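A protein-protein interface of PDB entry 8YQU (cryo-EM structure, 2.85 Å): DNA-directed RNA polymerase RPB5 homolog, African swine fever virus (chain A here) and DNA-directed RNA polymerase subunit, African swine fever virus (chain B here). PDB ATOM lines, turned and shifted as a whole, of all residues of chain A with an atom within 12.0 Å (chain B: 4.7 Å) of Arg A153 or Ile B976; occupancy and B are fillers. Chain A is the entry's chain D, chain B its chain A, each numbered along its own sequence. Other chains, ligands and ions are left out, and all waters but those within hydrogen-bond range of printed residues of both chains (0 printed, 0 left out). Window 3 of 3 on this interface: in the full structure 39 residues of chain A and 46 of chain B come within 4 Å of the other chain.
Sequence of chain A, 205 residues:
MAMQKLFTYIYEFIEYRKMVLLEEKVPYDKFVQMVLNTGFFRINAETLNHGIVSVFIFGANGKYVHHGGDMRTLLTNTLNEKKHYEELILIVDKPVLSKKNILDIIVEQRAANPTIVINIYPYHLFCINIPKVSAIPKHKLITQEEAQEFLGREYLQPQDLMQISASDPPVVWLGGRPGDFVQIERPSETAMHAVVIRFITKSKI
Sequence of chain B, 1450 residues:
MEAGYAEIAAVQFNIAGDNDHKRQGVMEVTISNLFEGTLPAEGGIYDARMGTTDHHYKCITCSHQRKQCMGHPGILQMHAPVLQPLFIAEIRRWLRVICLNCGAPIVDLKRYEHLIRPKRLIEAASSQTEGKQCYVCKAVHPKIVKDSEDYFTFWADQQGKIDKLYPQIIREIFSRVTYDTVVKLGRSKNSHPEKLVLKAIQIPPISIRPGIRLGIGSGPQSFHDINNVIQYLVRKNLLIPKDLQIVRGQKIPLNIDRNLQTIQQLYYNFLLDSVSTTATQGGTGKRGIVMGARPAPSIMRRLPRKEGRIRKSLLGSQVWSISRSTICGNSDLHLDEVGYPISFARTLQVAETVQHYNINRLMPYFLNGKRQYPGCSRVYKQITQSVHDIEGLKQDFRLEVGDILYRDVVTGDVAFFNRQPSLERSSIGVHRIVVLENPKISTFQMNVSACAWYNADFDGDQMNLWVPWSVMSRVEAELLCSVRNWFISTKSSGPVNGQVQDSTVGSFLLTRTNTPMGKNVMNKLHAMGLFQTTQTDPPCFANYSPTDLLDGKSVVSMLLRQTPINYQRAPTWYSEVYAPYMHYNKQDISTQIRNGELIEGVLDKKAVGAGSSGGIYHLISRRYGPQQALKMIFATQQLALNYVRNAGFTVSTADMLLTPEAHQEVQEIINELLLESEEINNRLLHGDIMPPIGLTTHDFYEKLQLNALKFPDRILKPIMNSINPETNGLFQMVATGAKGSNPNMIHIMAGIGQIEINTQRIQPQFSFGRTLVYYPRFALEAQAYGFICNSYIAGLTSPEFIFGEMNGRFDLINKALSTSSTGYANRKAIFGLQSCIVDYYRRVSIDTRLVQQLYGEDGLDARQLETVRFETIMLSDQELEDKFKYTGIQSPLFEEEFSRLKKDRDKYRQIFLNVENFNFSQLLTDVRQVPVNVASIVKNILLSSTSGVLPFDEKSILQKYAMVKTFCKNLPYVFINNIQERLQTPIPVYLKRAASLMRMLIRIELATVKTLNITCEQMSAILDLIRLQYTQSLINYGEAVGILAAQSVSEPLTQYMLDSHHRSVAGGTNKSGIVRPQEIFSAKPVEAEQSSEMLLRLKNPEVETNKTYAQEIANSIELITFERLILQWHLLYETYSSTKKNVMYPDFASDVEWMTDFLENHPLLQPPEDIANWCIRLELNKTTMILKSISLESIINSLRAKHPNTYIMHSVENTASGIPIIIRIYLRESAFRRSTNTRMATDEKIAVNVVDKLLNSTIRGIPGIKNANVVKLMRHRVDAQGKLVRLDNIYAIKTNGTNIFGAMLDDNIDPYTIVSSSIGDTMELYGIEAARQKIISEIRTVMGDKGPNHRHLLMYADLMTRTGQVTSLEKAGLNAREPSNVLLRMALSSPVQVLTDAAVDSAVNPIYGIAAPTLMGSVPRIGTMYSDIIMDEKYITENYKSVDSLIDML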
ATOM      1  N   GLN A 144      -9.324  17.733   1.375  1.00  0.00           N
ATOM      2  CA  GLN A 144      -9.952  16.672   0.595  1.00  0.00           C
ATOM      3  C   GLN A 144     -11.445  16.916   0.418  1.00  0.00           C
ATOM      4  O   GLN A 144     -12.000  16.629  -0.647  1.00  0.00           O
ATOM      5  CB  GLN A 144      -9.707  15.317   1.256  1.00  0.00           C
ATOM      6  CG  GLN A 144      -8.259  14.861   1.228  1.00  0.00           C
ATOM      7  CD  GLN A 144      -7.737  14.674  -0.182  1.00  0.00           C
ATOM      8  OE1 GLN A 144      -6.715  15.247  -0.560  1.00  0.00           O
ATOM      9  NE2 GLN A 144      -8.441  13.871  -0.971  1.00  0.00           N
ATOM     10  N   GLU A 145     -12.115  17.429   1.452  1.00  0.00           N
ATOM     11  CA  GLU A 145     -13.557  17.641   1.368  1.00  0.00           C
ATOM     12  C   GLU A 145     -13.912  18.699   0.328  1.00  0.00           C
ATOM     13  O   GLU A 145     -14.867  18.528  -0.439  1.00  0.00           O
ATOM     14  CB  GLU A 145     -14.112  18.022   2.742  1.00  0.00           C
ATOM     15  CG  GLU A 145     -14.210  16.868   3.746  1.00  0.00           C
ATOM     16  CD  GLU A 145     -12.867  16.402   4.298  1.00  0.00           C
ATOM     17  OE1 GLU A 145     -11.816  16.678   3.682  1.00  0.00           O
ATOM     18  OE2 GLU A 145     -12.865  15.752   5.363  1.00  0.00           O
ATOM     19  N   GLU A 146     -13.159  19.802   0.289  1.00  0.00           N
ATOM     20  CA  GLU A 146     -13.421  20.837  -0.708  1.00  0.00           C
ATOM     21  C   GLU A 146     -13.197  20.310  -2.120  1.00  0.00           C
ATOM     22  O   GLU A 146     -13.990  20.586  -3.029  1.00  0.00           O
ATOM     23  CB  GLU A 146     -12.539  22.056  -0.446  1.00  0.00           C
ATOM     24  CG  GLU A 146     -12.877  22.804   0.831  1.00  0.00           C
ATOM     25  CD  GLU A 146     -12.188  24.152   0.915  1.00  0.00           C
ATOM     26  OE1 GLU A 146     -11.070  24.285   0.375  1.00  0.00           O
ATOM     27  OE2 GLU A 146     -12.766  25.079   1.519  1.00  0.00           O
ATOM     28  N   ALA A 147     -12.120  19.551  -2.321  1.00  0.00           N
ATOM     29  CA  ALA A 147     -11.858  18.971  -3.634  1.00  0.00           C
ATOM     30  C   ALA A 147     -12.950  17.988  -4.028  1.00  0.00           C
ATOM     31  O   ALA A 147     -13.357  17.939  -5.193  1.00  0.00           O
ATOM     32  CB  ALA A 147     -10.491  18.290  -3.643  1.00  0.00           C
ATOM     33  N   GLN A 148     -13.430  17.189  -3.074  1.00  0.00           N
ATOM     34  CA  GLN A 148     -14.507  16.251  -3.372  1.00  0.00           C
ATOM     35  C   GLN A 148     -15.789  16.981  -3.744  1.00  0.00           C
ATOM     36  O   GLN A 148     -16.498  16.564  -4.666  1.00  0.00           O
ATOM     37  CB  GLN A 148     -14.744  15.316  -2.185  1.00  0.00           C
ATOM     38  CG  GLN A 148     -13.655  14.269  -1.984  1.00  0.00           C
ATOM     39  CD  GLN A 148     -13.306  13.520  -3.258  1.00  0.00           C
ATOM     40  OE1 GLN A 148     -12.134  13.272  -3.542  1.00  0.00           O
ATOM     41  NE2 GLN A 148     -14.325  13.131  -4.018  1.00  0.00           N
ATOM     42  N   GLU A 149     -16.105  18.074  -3.045  1.00  0.00           N
ATOM     43  CA  GLU A 149     -17.270  18.872  -3.419  1.00  0.00           C
ATOM     44  C   GLU A 149     -17.117  19.442  -4.824  1.00  0.00           C
ATOM     45  O   GLU A 149     -18.055  19.391  -5.633  1.00  0.00           O
ATOM     46  CB  GLU A 149     -17.484  19.999  -2.407  1.00  0.00           C
ATOM     47  CG  GLU A 149     -18.026  19.538  -1.067  1.00  0.00           C
ATOM     48  CD  GLU A 149     -19.452  19.030  -1.157  1.00  0.00           C
ATOM     49  OE1 GLU A 149     -20.226  19.572  -1.973  1.00  0.00           O
ATOM     50  OE2 GLU A 149     -19.797  18.091  -0.411  1.00  0.00           O
ATOM     51  N   PHE A 150     -15.933  19.977  -5.135  1.00  0.00           N
ATOM     52  CA  PHE A 150     -15.700  20.552  -6.456  1.00  0.00           C
ATOM     53  C   PHE A 150     -15.830  19.502  -7.551  1.00  0.00           C
ATOM     54  O   PHE A 150     -16.437  19.758  -8.598  1.00  0.00           O
ATOM     55  CB  PHE A 150     -14.321  21.207  -6.503  1.00  0.00           C
ATOM     56  CG  PHE A 150     -13.869  21.566  -7.886  1.00  0.00           C
ATOM     57  CD1 PHE A 150     -14.489  22.586  -8.588  1.00  0.00           C
ATOM     58  CD2 PHE A 150     -12.829  20.881  -8.490  1.00  0.00           C
ATOM     59  CE1 PHE A 150     -14.076  22.918  -9.862  1.00  0.00           C
ATOM     60  CE2 PHE A 150     -12.414  21.208  -9.764  1.00  0.00           C
ATOM     61  CZ  PHE A 150     -13.037  22.228 -10.451  1.00  0.00           C
ATOM     62  N   LEU A 151     -15.269  18.311  -7.329  1.00  0.00           N
ATOM     63  CA  LEU A 151     -15.353  17.257  -8.332  1.00  0.00           C
ATOM     64  C   LEU A 151     -16.767  16.706  -8.456  1.00  0.00           C
ATOM     65  O   LEU A 151     -17.191  16.337  -9.557  1.00  0.00           O
ATOM     66  CB  LEU A 151     -14.373  16.132  -8.000  1.00  0.00           C
ATOM     67  CG  LEU A 151     -12.891  16.509  -7.960  1.00  0.00           C
ATOM     68  CD1 LEU A 151     -12.053  15.339  -7.476  1.00  0.00           C
ATOM     69  CD2 LEU A 151     -12.419  16.981  -9.323  1.00  0.00           C
ATOM     70  N   GLY A 152     -17.508  16.636  -7.349  1.00  0.00           N
ATOM     71  CA  GLY A 152     -18.883  16.178  -7.421  1.00  0.00           C
ATOM     72  C   GLY A 152     -19.775  17.138  -8.180  1.00  0.00           C
ATOM     73  O   GLY A 152     -20.659  16.715  -8.930  1.00  0.00           O
ATOM     74  N   ARG A 153     -19.562  18.443  -7.996  1.00  0.00           N
ATOM     75  CA  ARG A 153     -20.337  19.416  -8.761  1.00  0.00           C
ATOM     76  C   ARG A 153     -20.024  19.323 -10.250  1.00  0.00           C
ATOM     77  O   ARG A 153     -20.923  19.450 -11.088  1.00  0.00           O
ATOM     78  CB  ARG A 153     -20.072  20.831  -8.248  1.00  0.00           C
ATOM     79  CG  ARG A 153     -21.054  21.863  -8.780  1.00  0.00           C
ATOM     80  CD  ARG A 153     -20.450  22.679  -9.910  1.00  0.00           C
ATOM     81  NE  ARG A 153     -21.408  23.617 -10.479  1.00  0.00           N
ATOM     82  CZ  ARG A 153     -21.231  24.266 -11.622  1.00  0.00           C
ATOM     83  NH1 ARG A 153     -20.140  24.098 -12.351  1.00  0.00           N
ATOM     84  NH2 ARG A 153     -22.174  25.104 -12.044  1.00  0.00           N
ATOM     85  N   GLU A 154     -18.759  19.098 -10.596  1.00  0.00           N
ATOM     86  CA  GLU A 154     -18.308  19.113 -11.981  1.00  0.00           C
ATOM     87  C   GLU A 154     -18.327  17.740 -12.640  1.00  0.00           C
ATOM     88  O   GLU A 154     -17.931  17.631 -13.805  1.00  0.00           O
ATOM     89  CB  GLU A 154     -16.892  19.692 -12.062  1.00  0.00           C
ATOM     90  CG  GLU A 154     -16.776  21.122 -11.571  1.00  0.00           C
ATOM     91  CD  GLU A 154     -16.986  22.135 -12.677  1.00  0.00           C
ATOM     92  OE1 GLU A 154     -16.430  21.938 -13.778  1.00  0.00           O
ATOM     93  OE2 GLU A 154     -17.706  23.129 -12.445  1.00  0.00           O
ATOM     94  N   TYR A 155     -18.776  16.702 -11.933  1.00  0.00           N
ATOM     95  CA  TYR A 155     -18.784  15.332 -12.452  1.00  0.00           C
ATOM     96  C   TYR A 155     -17.393  14.922 -12.932  1.00  0.00           C
ATOM     97  O   TYR A 155     -17.219  14.363 -14.016  1.00  0.00           O
ATOM     98  CB  TYR A 155     -19.816  15.172 -13.571  1.00  0.00           C
ATOM     99  CG  TYR A 155     -21.234  14.978 -13.090  1.00  0.00           C
ATOM    100  CD1 TYR A 155     -21.631  13.787 -12.500  1.00  0.00           C
ATOM    101  CD2 TYR A 155     -22.180  15.984 -13.232  1.00  0.00           C
ATOM    102  CE1 TYR A 155     -22.928  13.605 -12.060  1.00  0.00           C
ATOM    103  CE2 TYR A 155     -23.478  15.811 -12.797  1.00  0.00           C
ATOM    104  CZ  TYR A 155     -23.846  14.620 -12.212  1.00  0.00           C
ATOM    105  OH  TYR A 155     -25.139  14.443 -11.777  1.00  0.00           O
ATOM    106  N   LEU A 156     -16.391  15.207 -12.106  1.00  0.00           N
ATOM    107  CA  LEU A 156     -15.000  14.996 -12.471  1.00  0.00           C
ATOM    108  C   LEU A 156     -14.334  14.004 -11.528  1.00  0.00           C
ATOM    109  O   LEU A 156     -14.763  13.803 -10.389  1.00  0.00           O
ATOM    110  CB  LEU A 156     -14.217  16.315 -12.460  1.00  0.00           C
ATOM    111  CG  LEU A 156     -14.371  17.213 -13.684  1.00  0.00           C
ATOM    112  CD1 LEU A 156     -13.580  18.496 -13.502  1.00  0.00           C
ATOM    113  CD2 LEU A 156     -13.930  16.476 -14.937  1.00  0.00           C
ATOM    114  N   GLN A 157     -13.275  13.385 -12.030  1.00  0.00           N
ATOM    115  CA  GLN A 157     -12.395  12.511 -11.279  1.00  0.00           C
ATOM    116  C   GLN A 157     -11.061  13.201 -11.033  1.00  0.00           C
ATOM    117  O   GLN A 157     -10.678  14.113 -11.773  1.00  0.00           O
ATOM    118  CB  GLN A 157     -12.160  11.195 -12.036  1.00  0.00           C
ATOM    119  CG  GLN A 157     -13.410  10.367 -12.263  1.00  0.00           C
ATOM    120  CD  GLN A 157     -14.090   9.973 -10.969  1.00  0.00           C
ATOM    121  OE1 GLN A 157     -15.235  10.347 -10.717  1.00  0.00           O
ATOM    122  NE2 GLN A 157     -13.383   9.215 -10.139  1.00  0.00           N
ATOM    123  N   PRO A 158     -10.328  12.804  -9.989  1.00  0.00           N
ATOM    124  CA  PRO A 158      -9.007  13.410  -9.759  1.00  0.00           C
ATOM    125  C   PRO A 158      -8.049  13.223 -10.922  1.00  0.00           C
ATOM    126  O   PRO A 158      -7.147  14.049 -11.108  1.00  0.00           O
ATOM    127  CB  PRO A 158      -8.512  12.693  -8.496  1.00  0.00           C
ATOM    128  CG  PRO A 158      -9.755  12.264  -7.801  1.00  0.00           C
ATOM    129  CD  PRO A 158     -10.721  11.906  -8.890  1.00  0.00           C
ATOM    130  N   ASP A 160      -8.860  13.516 -14.010  1.00  0.00           N
ATOM    131  CA  ASP A 160      -9.279  14.374 -15.110  1.00  0.00           C
ATOM    132  C   ASP A 160      -8.757  15.798 -14.994  1.00  0.00           C
ATOM    133  O   ASP A 160      -8.643  16.486 -16.015  1.00  0.00           O
ATOM    134  CB  ASP A 160     -10.807  14.407 -15.202  1.00  0.00           C
ATOM    135  CG  ASP A 160     -11.401  13.050 -15.519  1.00  0.00           C
ATOM    136  OD1 ASP A 160     -10.637  12.138 -15.897  1.00  0.00           O
ATOM    137  OD2 ASP A 160     -12.633  12.895 -15.393  1.00  0.00           O
ATOM    138  N   LEU A 161      -8.438  16.254 -13.787  1.00  0.00           N
ATOM    139  CA  LEU A 161      -7.925  17.601 -13.600  1.00  0.00           C
ATOM    140  C   LEU A 161      -6.510  17.719 -14.158  1.00  0.00           C
ATOM    141  O   LEU A 161      -5.851  16.725 -14.474  1.00  0.00           O
ATOM    142  CB  LEU A 161      -7.919  17.974 -12.119  1.00  0.00           C
ATOM    143  CG  LEU A 161      -9.256  18.001 -11.380  1.00  0.00           C
ATOM    144  CD1 LEU A 161      -9.018  18.208  -9.895  1.00  0.00           C
ATOM    145  CD2 LEU A 161     -10.155  19.088 -11.936  1.00  0.00           C
ATOM    146  N   PHE A 181      -4.587  18.214  -3.576  1.00  0.00           N
ATOM    147  CA  PHE A 181      -5.116  19.179  -4.530  1.00  0.00           C
ATOM    148  C   PHE A 181      -4.631  20.575  -4.172  1.00  0.00           C
ATOM    149  O   PHE A 181      -4.688  20.980  -3.004  1.00  0.00           O
ATOM    150  CB  PHE A 181      -6.646  19.142  -4.566  1.00  0.00           C
ATOM    151  CG  PHE A 181      -7.214  17.821  -5.002  1.00  0.00           C
ATOM    152  CD1 PHE A 181      -7.363  16.782  -4.101  1.00  0.00           C
ATOM    153  CD2 PHE A 181      -7.605  17.626  -6.315  1.00  0.00           C
ATOM    154  CE1 PHE A 181      -7.887  15.569  -4.504  1.00  0.00           C
ATOM    155  CE2 PHE A 181      -8.129  16.417  -6.722  1.00  0.00           C
ATOM    156  CZ  PHE A 181      -8.270  15.387  -5.816  1.00  0.00           C
ATOM    157  N   VAL A 195      -8.910  31.004 -11.574  1.00  0.00           N
ATOM    158  CA  VAL A 195      -8.686  30.033 -10.510  1.00  0.00           C
ATOM    159  C   VAL A 195      -8.760  28.641 -11.116  1.00  0.00           C
ATOM    160  O   VAL A 195      -9.748  28.302 -11.778  1.00  0.00           O
ATOM    161  CB  VAL A 195      -9.711  30.179  -9.373  1.00  0.00           C
ATOM    162  CG1 VAL A 195      -9.652  28.977  -8.451  1.00  0.00           C
ATOM    163  CG2 VAL A 195      -9.460  31.457  -8.599  1.00  0.00           C
ATOM    164  N   ILE A 197      -7.613  24.263 -10.338  1.00  0.00           N
ATOM    165  CA  ILE A 197      -7.302  23.258  -9.328  1.00  0.00           C
ATOM    166  C   ILE A 197      -6.499  22.151  -9.990  1.00  0.00           C
ATOM    167  O   ILE A 197      -6.902  21.625 -11.033  1.00  0.00           O
ATOM    168  CB  ILE A 197      -8.574  22.695  -8.667  1.00  0.00           C
ATOM    169  CG1 ILE A 197      -9.288  23.794  -7.880  1.00  0.00           C
ATOM    170  CG2 ILE A 197      -8.229  21.533  -7.753  1.00  0.00           C
ATOM    171  CD1 ILE A 197     -10.596  23.358  -7.270  1.00  0.00           C
ATOM    172  N   TYR B 841     -19.701  22.404 -19.718  1.00  0.00           N
ATOM    173  CA  TYR B 841     -19.338  23.304 -18.634  1.00  0.00           C
ATOM    174  C   TYR B 841     -18.509  24.486 -19.116  1.00  0.00           C
ATOM    175  O   TYR B 841     -17.966  25.226 -18.290  1.00  0.00           O
ATOM    176  CB  TYR B 841     -18.571  22.545 -17.551  1.00  0.00           C
ATOM    177  CG  TYR B 841     -19.420  21.649 -16.679  1.00  0.00           C
ATOM    178  CD1 TYR B 841     -19.689  20.339 -17.051  1.00  0.00           C
ATOM    179  CD2 TYR B 841     -19.938  22.109 -15.478  1.00  0.00           C
ATOM    180  CE1 TYR B 841     -20.459  19.516 -16.255  1.00  0.00           C
ATOM    181  CE2 TYR B 841     -20.708  21.291 -14.675  1.00  0.00           C
ATOM    182  CZ  TYR B 841     -20.965  19.997 -15.068  1.00  0.00           C
ATOM    183  OH  TYR B 841     -21.733  19.181 -14.270  1.00  0.00           O
ATOM    184  N   PRO B 972     -22.576  35.915 -12.172  1.00  0.00           N
ATOM    185  CA  PRO B 972     -21.975  34.625 -12.556  1.00  0.00           C
ATOM    186  C   PRO B 972     -22.978  33.569 -12.999  1.00  0.00           C
ATOM    187  O   PRO B 972     -22.561  32.574 -13.604  1.00  0.00           O
ATOM    188  CB  PRO B 972     -21.241  34.187 -11.283  1.00  0.00           C
ATOM    189  CG  PRO B 972     -20.931  35.452 -10.591  1.00  0.00           C
ATOM    190  CD  PRO B 972     -22.118  36.333 -10.835  1.00  0.00           C
ATOM    191  N   TYR B 973     -24.271  33.741 -12.719  1.00  0.00           N
ATOM    192  CA  TYR B 973     -25.267  32.776 -13.173  1.00  0.00           C
ATOM    193  C   TYR B 973     -25.475  32.802 -14.680  1.00  0.00           C
ATOM    194  O   TYR B 973     -26.176  31.930 -15.203  1.00  0.00           O
ATOM    195  CB  TYR B 973     -26.601  33.013 -12.466  1.00  0.00           C
ATOM    196  CG  TYR B 973     -26.605  32.593 -11.016  1.00  0.00           C
ATOM    197  CD1 TYR B 973     -26.541  31.253 -10.663  1.00  0.00           C
ATOM    198  CD2 TYR B 973     -26.679  33.535 -10.000  1.00  0.00           C
ATOM    199  CE1 TYR B 973     -26.548  30.863  -9.340  1.00  0.00           C
ATOM    200  CE2 TYR B 973     -26.687  33.153  -8.674  1.00  0.00           C
ATOM    201  CZ  TYR B 973     -26.620  31.817  -8.350  1.00  0.00           C
ATOM    202  OH  TYR B 973     -26.626  31.431  -7.030  1.00  0.00           O
ATOM    203  N   VAL B 974     -24.904  33.783 -15.385  1.00  0.00           N
ATOM    204  CA  VAL B 974     -24.948  33.777 -16.844  1.00  0.00           C
ATOM    205  C   VAL B 974     -24.284  32.523 -17.392  1.00  0.00           C
ATOM    206  O   VAL B 974     -24.689  31.999 -18.438  1.00  0.00           O
ATOM    207  CB  VAL B 974     -24.294  35.060 -17.397  1.00  0.00           C
ATOM    208  CG1 VAL B 974     -24.217  35.020 -18.911  1.00  0.00           C
ATOM    209  CG2 VAL B 974     -25.073  36.283 -16.947  1.00  0.00           C
ATOM    210  N   PHE B 975     -23.277  32.007 -16.691  1.00  0.00           N
ATOM    211  CA  PHE B 975     -22.560  30.823 -17.138  1.00  0.00           C
ATOM    212  C   PHE B 975     -23.290  29.521 -16.845  1.00  0.00           C
ATOM    213  O   PHE B 975     -22.840  28.469 -17.312  1.00  0.00           O
ATOM    214  CB  PHE B 975     -21.174  30.768 -16.492  1.00  0.00           C
ATOM    215  CG  PHE B 975     -20.266  31.886 -16.906  1.00  0.00           C
ATOM    216  CD1 PHE B 975     -19.620  31.855 -18.128  1.00  0.00           C
ATOM    217  CD2 PHE B 975     -20.059  32.971 -16.073  1.00  0.00           C
ATOM    218  CE1 PHE B 975     -18.783  32.880 -18.510  1.00  0.00           C
ATOM    219  CE2 PHE B 975     -19.224  34.001 -16.451  1.00  0.00           C
ATOM    220  CZ  PHE B 975     -18.585  33.955 -17.672  1.00  0.00           C
ATOM    221  N   ILE B 976     -24.391  29.543 -16.092  1.00  0.00           N
ATOM    222  CA  ILE B 976     -25.031  28.279 -15.745  1.00  0.00           C
ATOM    223  C   ILE B 976     -26.412  28.171 -16.379  1.00  0.00           C
ATOM    224  O   ILE B 976     -26.592  27.437 -17.356  1.00  0.00           O
ATOM    225  CB  ILE B 976     -25.121  28.132 -14.216  1.00  0.00           C
ATOM    226  CG1 ILE B 976     -23.755  28.377 -13.574  1.00  0.00           C
ATOM    227  CG2 ILE B 976     -25.643  26.761 -13.833  1.00  0.00           C
ATOM    228  CD1 ILE B 976     -23.806  28.536 -12.074  1.00  0.00           C
ATOM    229  N   ASN B 977     -27.378  28.935 -15.862  1.00  0.00           N
ATOM    230  CA  ASN B 977     -28.735  28.997 -16.405  1.00  0.00           C
ATOM    231  C   ASN B 977     -29.591  29.933 -15.562  1.00  0.00           C
ATOM    232  O   ASN B 977     -29.106  30.514 -14.587  1.00  0.00           O
ATOM    233  CB  ASN B 977     -29.391  27.614 -16.477  1.00  0.00           C
ATOM    234  CG  ASN B 977     -29.296  26.858 -15.178  1.00  0.00           C
ATOM    235  OD1 ASN B 977     -28.786  27.373 -14.188  1.00  0.00           O
ATOM    236  ND2 ASN B 977     -29.788  25.626 -15.173  1.00  0.00           N
ATOM    237  N   GLN B 980     -30.777  27.840 -11.796  1.00  0.00           N
ATOM    238  CA  GLN B 980     -29.995  27.939 -10.569  1.00  0.00           C
ATOM    239  C   GLN B 980     -30.014  29.354 -10.007  1.00  0.00           C
ATOM    240  O   GLN B 980     -29.873  29.536  -8.792  1.00  0.00           O
ATOM    241  CB  GLN B 980     -28.558  27.481 -10.814  1.00  0.00           C
ATOM    242  CG  GLN B 980     -28.437  26.091 -11.419  1.00  0.00           C
ATOM    243  CD  GLN B 980     -29.107  25.021 -10.585  1.00  0.00           C
ATOM    244  OE1 GLN B 980     -28.988  25.009  -9.362  1.00  0.00           O
ATOM    245  NE2 GLN B 980     -29.815  24.115 -11.245  1.00  0.00           N
ATOM    246  N   PRO B 988     -19.672  28.226  -8.256  1.00  0.00           N
ATOM    247  CA  PRO B 988     -18.275  27.795  -8.140  1.00  0.00           C
ATOM    248  C   PRO B 988     -17.328  28.984  -8.133  1.00  0.00           C
ATOM    249  O   PRO B 988     -17.618  30.042  -8.694  1.00  0.00           O
ATOM    250  CB  PRO B 988     -18.068  26.922  -9.381  1.00  0.00           C
ATOM    251  CG  PRO B 988     -19.429  26.455  -9.739  1.00  0.00           C
ATOM    252  CD  PRO B 988     -20.354  27.579  -9.388  1.00  0.00           C
ATOM    253  N   TYR B 990     -14.386  29.415  -9.559  1.00  0.00           N
ATOM    254  CA  TYR B 990     -13.803  29.795 -10.842  1.00  0.00           C
ATOM    255  C   TYR B 990     -14.790  30.531 -11.737  1.00  0.00           C
ATOM    256  O   TYR B 990     -14.364  31.201 -12.683  1.00  0.00           O
ATOM    257  CB  TYR B 990     -13.255  28.564 -11.565  1.00  0.00           C
ATOM    258  CG  TYR B 990     -14.305  27.635 -12.130  1.00  0.00           C
ATOM    259  CD1 TYR B 990     -14.924  26.686 -11.331  1.00  0.00           C
ATOM    260  CD2 TYR B 990     -14.664  27.698 -13.469  1.00  0.00           C
ATOM    261  CE1 TYR B 990     -15.877  25.832 -11.847  1.00  0.00           C
ATOM    262  CE2 TYR B 990     -15.616  26.849 -13.993  1.00  0.00           C
ATOM    263  CZ  TYR B 990     -16.219  25.919 -13.178  1.00  0.00           C
ATOM    264  OH  TYR B 990     -17.170  25.071 -13.697  1.00  0.00           O
ATOM    265  N   LEU B 991     -16.092  30.426 -11.468  1.00  0.00           N
ATOM    266  CA  LEU B 991     -17.077  31.211 -12.201  1.00  0.00           C
ATOM    267  C   LEU B 991     -17.267  32.599 -11.611  1.00  0.00           C
ATOM    268  O   LEU B 991     -17.641  33.527 -12.337  1.00  0.00           O
ATOM    269  CB  LEU B 991     -18.423  30.482 -12.237  1.00  0.00           C
ATOM    270  CG  LEU B 991     -18.475  29.211 -13.084  1.00  0.00           C
ATOM    271  CD1 LEU B 991     -19.881  28.641 -13.101  1.00  0.00           C
ATOM    272  CD2 LEU B 991     -17.995  29.496 -14.495  1.00  0.00           C
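OH of Tyr B990 is in hydrogen-bond range of NH1 of Arg A153, at 3.4 Å.
The side-chain hydroxyl (OH) of Tyr B990 lies close to the side-chain carboxylate (OE1) of Glu A154 (3.2 Å).
OH of Tyr B841 is in hydrogen-bond range of O of Arg A153, 3.3 Å away.
OE2 of Glu A154 lies within salt-bridge range of NH1 of Arg A153.
Among the printed residues, pairs that only touch across the chains: Tyr A155 with Tyr B841 (3.4 Å), Arg A153 with Pro B988 (3.4 Å), Val A195 with Tyr B990 (3.5 Å), Arg A153 with Ile B976 (3.8 Å), Glu A154 with Tyr B841 (3.9 Å) and Phe A150 with Tyr B990 (3.96 Å).
Glu A149 touches none of the printed residues of chain B.
Arg A153 touches four residues of chain B.
Of the printed residues of chain B, Glu A154 touches Tyr B841 (3.9 Å) and Tyr B990 (2.4 Å).
Of the printed residues of chain B, Tyr A155 touches Tyr B841 (3.4 Å).
Asp A160 touches none of the printed residues of chain B.
Tyr B841 touches just these residues of chain A: Arg A153, Glu A154 and Tyr A155.
No residue of chain A comes within 4 Å of Tyr B973.
No residue of chain A comes within 4 Å of Phe B975.
Ile B976 touches just one residue of chain A: Arg A153.
No residue of chain A comes within 4 Å of Asn B977.
No residue of chain A comes within 4 Å of Gln B980.
Pro B988 touches just one residue of chain A: Arg A153 (3.4 Å).
Leu B991 touches none of the printed residues of chain A.
The nearest residue of chain B that does not touch Arg A153 is Leu B991 (4.3 Å).
The nearest residue of chain A that does not touch Ile B976 is Glu A154 (8.1 Å).
The nearest printed residue of chain B that does not touch Glu A154 is Pro B988 (4.6 Å).
Printed residues of chain A that touch a printed residue of chain B: Phe A150, Arg A153, Glu A154, Tyr A155 and Val A195.
Hydrophobic or aromatic side chains of chain A within 4 Å of the printed part of chain B: Phe A150 and Tyr A155.
Of the 11 printed residues of chain B, 4 touch a printed residue of chain A.
Hydrophobic or aromatic side chains of chain B that line the printed part of chain A: Tyr B841, Ile B976, Pro B988 and Tyr B990.
Among the printed residues, 9 pairs touch across the chains.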
